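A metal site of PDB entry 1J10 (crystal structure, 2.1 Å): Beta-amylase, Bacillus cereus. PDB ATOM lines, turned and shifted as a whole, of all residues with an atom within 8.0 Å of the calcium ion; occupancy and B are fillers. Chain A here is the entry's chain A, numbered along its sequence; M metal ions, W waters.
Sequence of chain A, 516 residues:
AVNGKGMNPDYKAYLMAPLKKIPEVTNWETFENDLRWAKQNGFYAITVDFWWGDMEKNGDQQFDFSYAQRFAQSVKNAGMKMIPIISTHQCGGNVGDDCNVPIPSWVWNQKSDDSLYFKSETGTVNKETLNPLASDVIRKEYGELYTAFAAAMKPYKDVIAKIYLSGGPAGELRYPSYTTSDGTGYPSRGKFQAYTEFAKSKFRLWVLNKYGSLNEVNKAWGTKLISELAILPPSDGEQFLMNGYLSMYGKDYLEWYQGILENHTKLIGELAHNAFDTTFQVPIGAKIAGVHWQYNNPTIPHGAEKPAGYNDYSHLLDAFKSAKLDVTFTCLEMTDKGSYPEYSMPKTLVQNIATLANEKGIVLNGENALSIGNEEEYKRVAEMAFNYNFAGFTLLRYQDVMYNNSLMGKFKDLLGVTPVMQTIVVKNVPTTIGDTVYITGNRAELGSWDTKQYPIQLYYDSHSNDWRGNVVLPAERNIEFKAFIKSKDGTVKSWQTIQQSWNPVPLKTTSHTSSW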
ATOM      1  N   TRP A  52       7.612  35.105  -5.528  1.00  0.00           N
ATOM      2  CA  TRP A  52       7.475  33.661  -5.683  1.00  0.00           C
ATOM      3  C   TRP A  52       6.002  33.315  -5.522  1.00  0.00           C
ATOM      4  O   TRP A  52       5.430  32.575  -6.317  1.00  0.00           O
ATOM      5  CB  TRP A  52       8.327  32.936  -4.634  1.00  0.00           C
ATOM      6  CG  TRP A  52       8.448  31.443  -4.856  1.00  0.00           C
ATOM      7  CD1 TRP A  52       8.065  30.741  -5.968  1.00  0.00           C
ATOM      8  CD2 TRP A  52       8.952  30.477  -3.924  1.00  0.00           C
ATOM      9  NE1 TRP A  52       8.294  29.400  -5.783  1.00  0.00           N
ATOM     10  CE2 TRP A  52       8.840  29.203  -4.537  1.00  0.00           C
ATOM     11  CE3 TRP A  52       9.491  30.550  -2.629  1.00  0.00           C
ATOM     12  CZ2 TRP A  52       9.245  28.025  -3.907  1.00  0.00           C
ATOM     13  CZ3 TRP A  52       9.888  29.383  -1.998  1.00  0.00           C
ATOM     14  CH2 TRP A  52       9.773  28.135  -2.637  1.00  0.00           C
ATOM     15  N   GLU A  56       4.458  31.046  -8.791  1.00  0.00           N
ATOM     16  CA  GLU A  56       4.272  29.595  -8.682  1.00  0.00           C
ATOM     17  C   GLU A  56       3.286  29.347  -7.556  1.00  0.00           C
ATOM     18  O   GLU A  56       3.451  28.449  -6.737  1.00  0.00           O
ATOM     19  CB  GLU A  56       5.616  28.913  -8.394  1.00  0.00           C
ATOM     20  CG  GLU A  56       5.598  27.401  -8.642  1.00  0.00           C
ATOM     21  CD  GLU A  56       6.925  26.729  -8.275  1.00  0.00           C
ATOM     22  OE1 GLU A  56       7.888  27.411  -7.878  1.00  0.00           O
ATOM     23  OE2 GLU A  56       6.988  25.494  -8.397  1.00  0.00           O
ATOM     24  N   GLY A  59       0.731  25.663  -7.492  1.00  0.00           N
ATOM     25  CA  GLY A  59       1.324  24.361  -7.254  1.00  0.00           C
ATOM     26  C   GLY A  59       2.672  24.209  -7.902  1.00  0.00           C
ATOM     27  O   GLY A  59       3.104  25.045  -8.706  1.00  0.00           O
ATOM     28  N   ASP A  60       3.350  23.118  -7.550  1.00  0.00           N
ATOM     29  CA  ASP A  60       4.663  22.803  -8.070  1.00  0.00           C
ATOM     30  C   ASP A  60       4.657  22.869  -9.590  1.00  0.00           C
ATOM     31  O   ASP A  60       3.837  22.223 -10.245  1.00  0.00           O
ATOM     32  CB  ASP A  60       5.077  21.397  -7.614  1.00  0.00           C
ATOM     33  CG  ASP A  60       6.539  21.096  -7.855  1.00  0.00           C
ATOM     34  OD1 ASP A  60       7.315  22.050  -8.046  1.00  0.00           O
ATOM     35  OD2 ASP A  60       6.908  19.915  -7.843  1.00  0.00           O
ATOM     36  N   GLN A  61       5.549  23.698 -10.129  1.00  0.00           N
ATOM     37  CA  GLN A  61       5.702  23.907 -11.569  1.00  0.00           C
ATOM     38  C   GLN A  61       4.526  24.566 -12.273  1.00  0.00           C
ATOM     39  O   GLN A  61       4.455  24.553 -13.500  1.00  0.00           O
ATOM     40  CB  GLN A  61       6.099  22.610 -12.274  1.00  0.00           C
ATOM     41  CG  GLN A  61       7.369  21.950 -11.751  1.00  0.00           C
ATOM     42  CD  GLN A  61       8.569  22.867 -11.777  1.00  0.00           C
ATOM     43  OE1 GLN A  61       8.805  23.630 -10.842  1.00  0.00           O
ATOM     44  NE2 GLN A  61       9.350  22.802 -12.851  1.00  0.00           N
ATOM     45  N   GLN A  62       3.586  25.116 -11.515  1.00  0.00           N
ATOM     46  CA  GLN A  62       2.450  25.816 -12.111  1.00  0.00           C
ATOM     47  C   GLN A  62       2.819  27.303 -12.095  1.00  0.00           C
ATOM     48  O   GLN A  62       2.361  28.071 -11.249  1.00  0.00           O
ATOM     49  CB  GLN A  62       1.174  25.535 -11.332  1.00  0.00           C
ATOM     50  CG  GLN A  62       0.770  24.071 -11.448  1.00  0.00           C
ATOM     51  CD  GLN A  62      -0.557  23.787 -10.801  1.00  0.00           C
ATOM     52  OE1 GLN A  62      -1.524  24.500 -11.018  1.00  0.00           O
ATOM     53  NE2 GLN A  62      -0.604  22.738  -9.990  1.00  0.00           N
ATOM     54  N   PHE A  63       3.715  27.650 -13.016  1.00  0.00           N
ATOM     55  CA  PHE A  63       4.256  28.999 -13.149  1.00  0.00           C
ATOM     56  C   PHE A  63       3.391  30.044 -13.847  1.00  0.00           C
ATOM     57  O   PHE A  63       2.575  29.724 -14.703  1.00  0.00           O
ATOM     58  CB  PHE A  63       5.593  28.938 -13.896  1.00  0.00           C
ATOM     59  CG  PHE A  63       6.639  28.127 -13.206  1.00  0.00           C
ATOM     60  CD1 PHE A  63       7.213  27.022 -13.834  1.00  0.00           C
ATOM     61  CD2 PHE A  63       7.106  28.500 -11.954  1.00  0.00           C
ATOM     62  CE1 PHE A  63       8.224  26.303 -13.214  1.00  0.00           C
ATOM     63  CE2 PHE A  63       8.109  27.792 -11.333  1.00  0.00           C
ATOM     64  CZ  PHE A  63       8.671  26.687 -11.968  1.00  0.00           C
ATOM     65  N   TRP A 106       1.645  25.541  -0.792  1.00  0.00           N
ATOM     66  CA  TRP A 106       1.920  24.125  -1.048  1.00  0.00           C
ATOM     67  C   TRP A 106       3.341  23.711  -0.676  1.00  0.00           C
ATOM     68  O   TRP A 106       3.614  22.522  -0.481  1.00  0.00           O
ATOM     69  CB  TRP A 106       1.643  23.770  -2.528  1.00  0.00           C
ATOM     70  CG  TRP A 106       2.475  24.554  -3.520  1.00  0.00           C
ATOM     71  CD1 TRP A 106       2.093  25.664  -4.210  1.00  0.00           C
ATOM     72  CD2 TRP A 106       3.834  24.282  -3.914  1.00  0.00           C
ATOM     73  NE1 TRP A 106       3.124  26.109  -4.992  1.00  0.00           N
ATOM     74  CE2 TRP A 106       4.203  25.288  -4.825  1.00  0.00           C
ATOM     75  CE3 TRP A 106       4.778  23.312  -3.567  1.00  0.00           C
ATOM     76  CZ2 TRP A 106       5.472  25.336  -5.408  1.00  0.00           C
ATOM     77  CZ3 TRP A 106       6.036  23.352  -4.145  1.00  0.00           C
ATOM     78  CH2 TRP A 106       6.374  24.362  -5.057  1.00  0.00           C
ATOM     79  N   VAL A 107       4.251  24.677  -0.604  1.00  0.00           N
ATOM     80  CA  VAL A 107       5.632  24.375  -0.260  1.00  0.00           C
ATOM     81  C   VAL A 107       5.757  23.816   1.163  1.00  0.00           C
ATOM     82  O   VAL A 107       6.494  22.869   1.403  1.00  0.00           O
ATOM     83  CB  VAL A 107       6.518  25.641  -0.428  1.00  0.00           C
ATOM     84  CG1 VAL A 107       7.948  25.335  -0.025  1.00  0.00           C
ATOM     85  CG2 VAL A 107       6.501  26.086  -1.877  1.00  0.00           C
ATOM     86  N   GLN A 110       5.640  20.038   1.704  1.00  0.00           N
ATOM     87  CA  GLN A 110       6.726  19.196   1.197  1.00  0.00           C
ATOM     88  C   GLN A 110       7.443  18.457   2.338  1.00  0.00           C
ATOM     89  O   GLN A 110       8.197  17.512   2.101  1.00  0.00           O
ATOM     90  CB  GLN A 110       7.778  20.027   0.444  1.00  0.00           C
ATOM     91  CG  GLN A 110       7.224  21.007  -0.592  1.00  0.00           C
ATOM     92  CD  GLN A 110       6.720  20.348  -1.853  1.00  0.00           C
ATOM     93  OE1 GLN A 110       5.565  19.920  -1.922  1.00  0.00           O
ATOM     94  NE2 GLN A 110       7.573  20.288  -2.867  1.00  0.00           N
ATOM     95  N   VAL A 137      15.099  21.087  -0.330  1.00  0.00           N
ATOM     96  CA  VAL A 137      13.911  21.736  -0.857  1.00  0.00           C
ATOM     97  C   VAL A 137      14.319  23.004  -1.594  1.00  0.00           C
ATOM     98  O   VAL A 137      13.799  23.323  -2.657  1.00  0.00           O
ATOM     99  CB  VAL A 137      12.923  22.087   0.265  1.00  0.00           C
ATOM    100  CG1 VAL A 137      11.683  22.745  -0.299  1.00  0.00           C
ATOM    101  CG2 VAL A 137      12.531  20.830   1.016  1.00  0.00           C
ATOM    102  N   LYS A 140      15.948  22.206  -5.042  1.00  0.00           N
ATOM    103  CA  LYS A 140      14.905  21.833  -5.984  1.00  0.00           C
ATOM    104  C   LYS A 140      14.050  23.019  -6.422  1.00  0.00           C
ATOM    105  O   LYS A 140      13.993  23.353  -7.611  1.00  0.00           O
ATOM    106  CB  LYS A 140      13.983  20.762  -5.389  1.00  0.00           C
ATOM    107  CG  LYS A 140      12.760  20.483  -6.245  1.00  0.00           C
ATOM    108  CD  LYS A 140      11.775  19.555  -5.560  1.00  0.00           C
ATOM    109  CE  LYS A 140      10.633  19.181  -6.512  1.00  0.00           C
ATOM    110  NZ  LYS A 140       9.663  20.284  -6.746  1.00  0.00           N
ATOM    111  N   GLU A 141      13.388  23.663  -5.464  1.00  0.00           N
ATOM    112  CA  GLU A 141      12.502  24.784  -5.751  1.00  0.00           C
ATOM    113  C   GLU A 141      13.143  26.036  -6.339  1.00  0.00           C
ATOM    114  O   GLU A 141      12.570  26.647  -7.236  1.00  0.00           O
ATOM    115  CB  GLU A 141      11.653  25.150  -4.529  1.00  0.00           C
ATOM    116  CG  GLU A 141      10.835  23.989  -3.953  1.00  0.00           C
ATOM    117  CD  GLU A 141       9.888  23.341  -4.961  1.00  0.00           C
ATOM    118  OE1 GLU A 141       9.537  23.969  -5.978  1.00  0.00           O
ATOM    119  OE2 GLU A 141       9.488  22.183  -4.729  1.00  0.00           O
ATOM    120  N   TYR A 142      14.331  26.423  -5.845  1.00  0.00           N
ATOM    121  CA  TYR A 142      15.010  27.603  -6.367  1.00  0.00           C
ATOM    122  C   TYR A 142      15.574  27.302  -7.732  1.00  0.00           C
ATOM    123  O   TYR A 142      15.495  28.127  -8.641  1.00  0.00           O
ATOM    124  CB  TYR A 142      16.133  28.077  -5.439  1.00  0.00           C
ATOM    125  CG  TYR A 142      15.669  28.811  -4.201  1.00  0.00           C
ATOM    126  CD1 TYR A 142      14.470  28.480  -3.555  1.00  0.00           C
ATOM    127  CD2 TYR A 142      16.458  29.823  -3.636  1.00  0.00           C
ATOM    128  CE1 TYR A 142      14.082  29.116  -2.388  1.00  0.00           C
ATOM    129  CE2 TYR A 142      16.074  30.461  -2.459  1.00  0.00           C
ATOM    130  CZ  TYR A 142      14.895  30.101  -1.837  1.00  0.00           C
ATOM    131  OH  TYR A 142      14.545  30.685  -0.651  1.00  0.00           O
ATOM    132  N   GLY A 143      16.157  26.118  -7.888  1.00  0.00           N
ATOM    133  CA  GLY A 143      16.697  25.734  -9.175  1.00  0.00           C
ATOM    134  C   GLY A 143      15.610  25.745 -10.227  1.00  0.00           C
ATOM    135  O   GLY A 143      15.818  26.228 -11.340  1.00  0.00           O
ATOM    136  N   GLU A 144      14.440  25.206  -9.884  1.00  0.00           N
ATOM    137  CA  GLU A 144      13.326  25.155 -10.809  1.00  0.00           C
ATOM    138  C   GLU A 144      12.830  26.541 -11.169  1.00  0.00           C
ATOM    139  O   GLU A 144      12.598  26.828 -12.345  1.00  0.00           O
ATOM    140  CB  GLU A 144      12.179  24.342 -10.209  1.00  0.00           C
ATOM    141  CG  GLU A 144      12.449  22.839 -10.211  1.00  0.00           C
ATOM    142  CD  GLU A 144      11.401  22.037  -9.465  1.00  0.00           C
ATOM    143  OE1 GLU A 144      10.664  22.598  -8.637  1.00  0.00           O
ATOM    144  OE2 GLU A 144      11.313  20.813  -9.710  1.00  0.00           O
ATOM    145  N   LEU A 145      12.702  27.397 -10.162  1.00  0.00           N
ATOM    146  CA  LEU A 145      12.224  28.760 -10.342  1.00  0.00           C
ATOM    147  C   LEU A 145      13.181  29.641 -11.158  1.00  0.00           C
ATOM    148  O   LEU A 145      12.758  30.369 -12.052  1.00  0.00           O
ATOM    149  CB  LEU A 145      11.958  29.395  -8.979  1.00  0.00           C
ATOM    150  CG  LEU A 145      11.347  30.801  -8.952  1.00  0.00           C
ATOM    151  CD1 LEU A 145       9.979  30.816  -9.599  1.00  0.00           C
ATOM    152  CD2 LEU A 145      11.274  31.256  -7.502  1.00  0.00           C
ATOM    153  N   ALA A 148      13.170  28.465 -14.769  1.00  0.00           N
ATOM    154  CA  ALA A 148      11.905  28.815 -15.428  1.00  0.00           C
ATOM    155  C   ALA A 148      11.844  30.306 -15.718  1.00  0.00           C
ATOM    156  O   ALA A 148      11.377  30.733 -16.777  1.00  0.00           O
ATOM    157  CB  ALA A 148      10.714  28.383 -14.585  1.00  0.00           C
HETATM  158 CA    CA M   1       8.838  24.009  -8.311  1.00  0.00          CA
HETATM  159  O   HOH W   1      10.263  26.100  -8.279  1.00  0.00           O
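The calcium ion is bound by the side-chain carboxylate (OE1) of Glu 144, 2.3 Å away. The side-chain carboxylate (OE2) of Glu 56 is bound to the calcium ion, 2.4 Å away. OE1 of Glu 141 is bound to the calcium ion (2.4 Å). The calcium ion is bound by OD1 of Asp 60 (2.5 Å). The calcium ion is bound by water W1. OE1 of Gln 61 binds the calcium ion, at 2.6 Å.
The side-chain carboxylate (OE2) of Glu 144 lies within salt-bridge range of the side-chain amino group (NZ) of Lys 140, at 3.4 Å. The indole nitrogen (NE1) of Trp 106 is in hydrogen-bond range of the backbone carbonyl oxygen (O) of Glu 56. NE1 of Trp 52 lies within hydrogen-bond range of OE1 of Glu 56. The side-chain carboxylate of Asp 60 is in salt-bridge range of the side-chain amino group of Lys 140, at 3.0 Å. OE2 of Glu 141 is in salt-bridge range of NZ of Lys 140 (2.8 Å). The side-chain amide nitrogen (NE2) of Gln 110 lies within hydrogen-bond range of the side-chain carboxylate (OE2) of Glu 141 (3.3 Å).
Within 4 Å of the calcium ion: Glu 56, Asp 60, Gln 61, Glu 141 and Glu 144. Along chain A the residues within 4 Å of the calcium ion span positions 56 to 144. The nearest printed residue that does not touch the calcium ion is Trp 106 (4.1 Å).
Water W1 lies within hydrogen-bond range of O of Glu 141 (2.6 Å), OE1 of Glu 56 (2.7 Å) and N of Leu 145 (3.3 Å).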
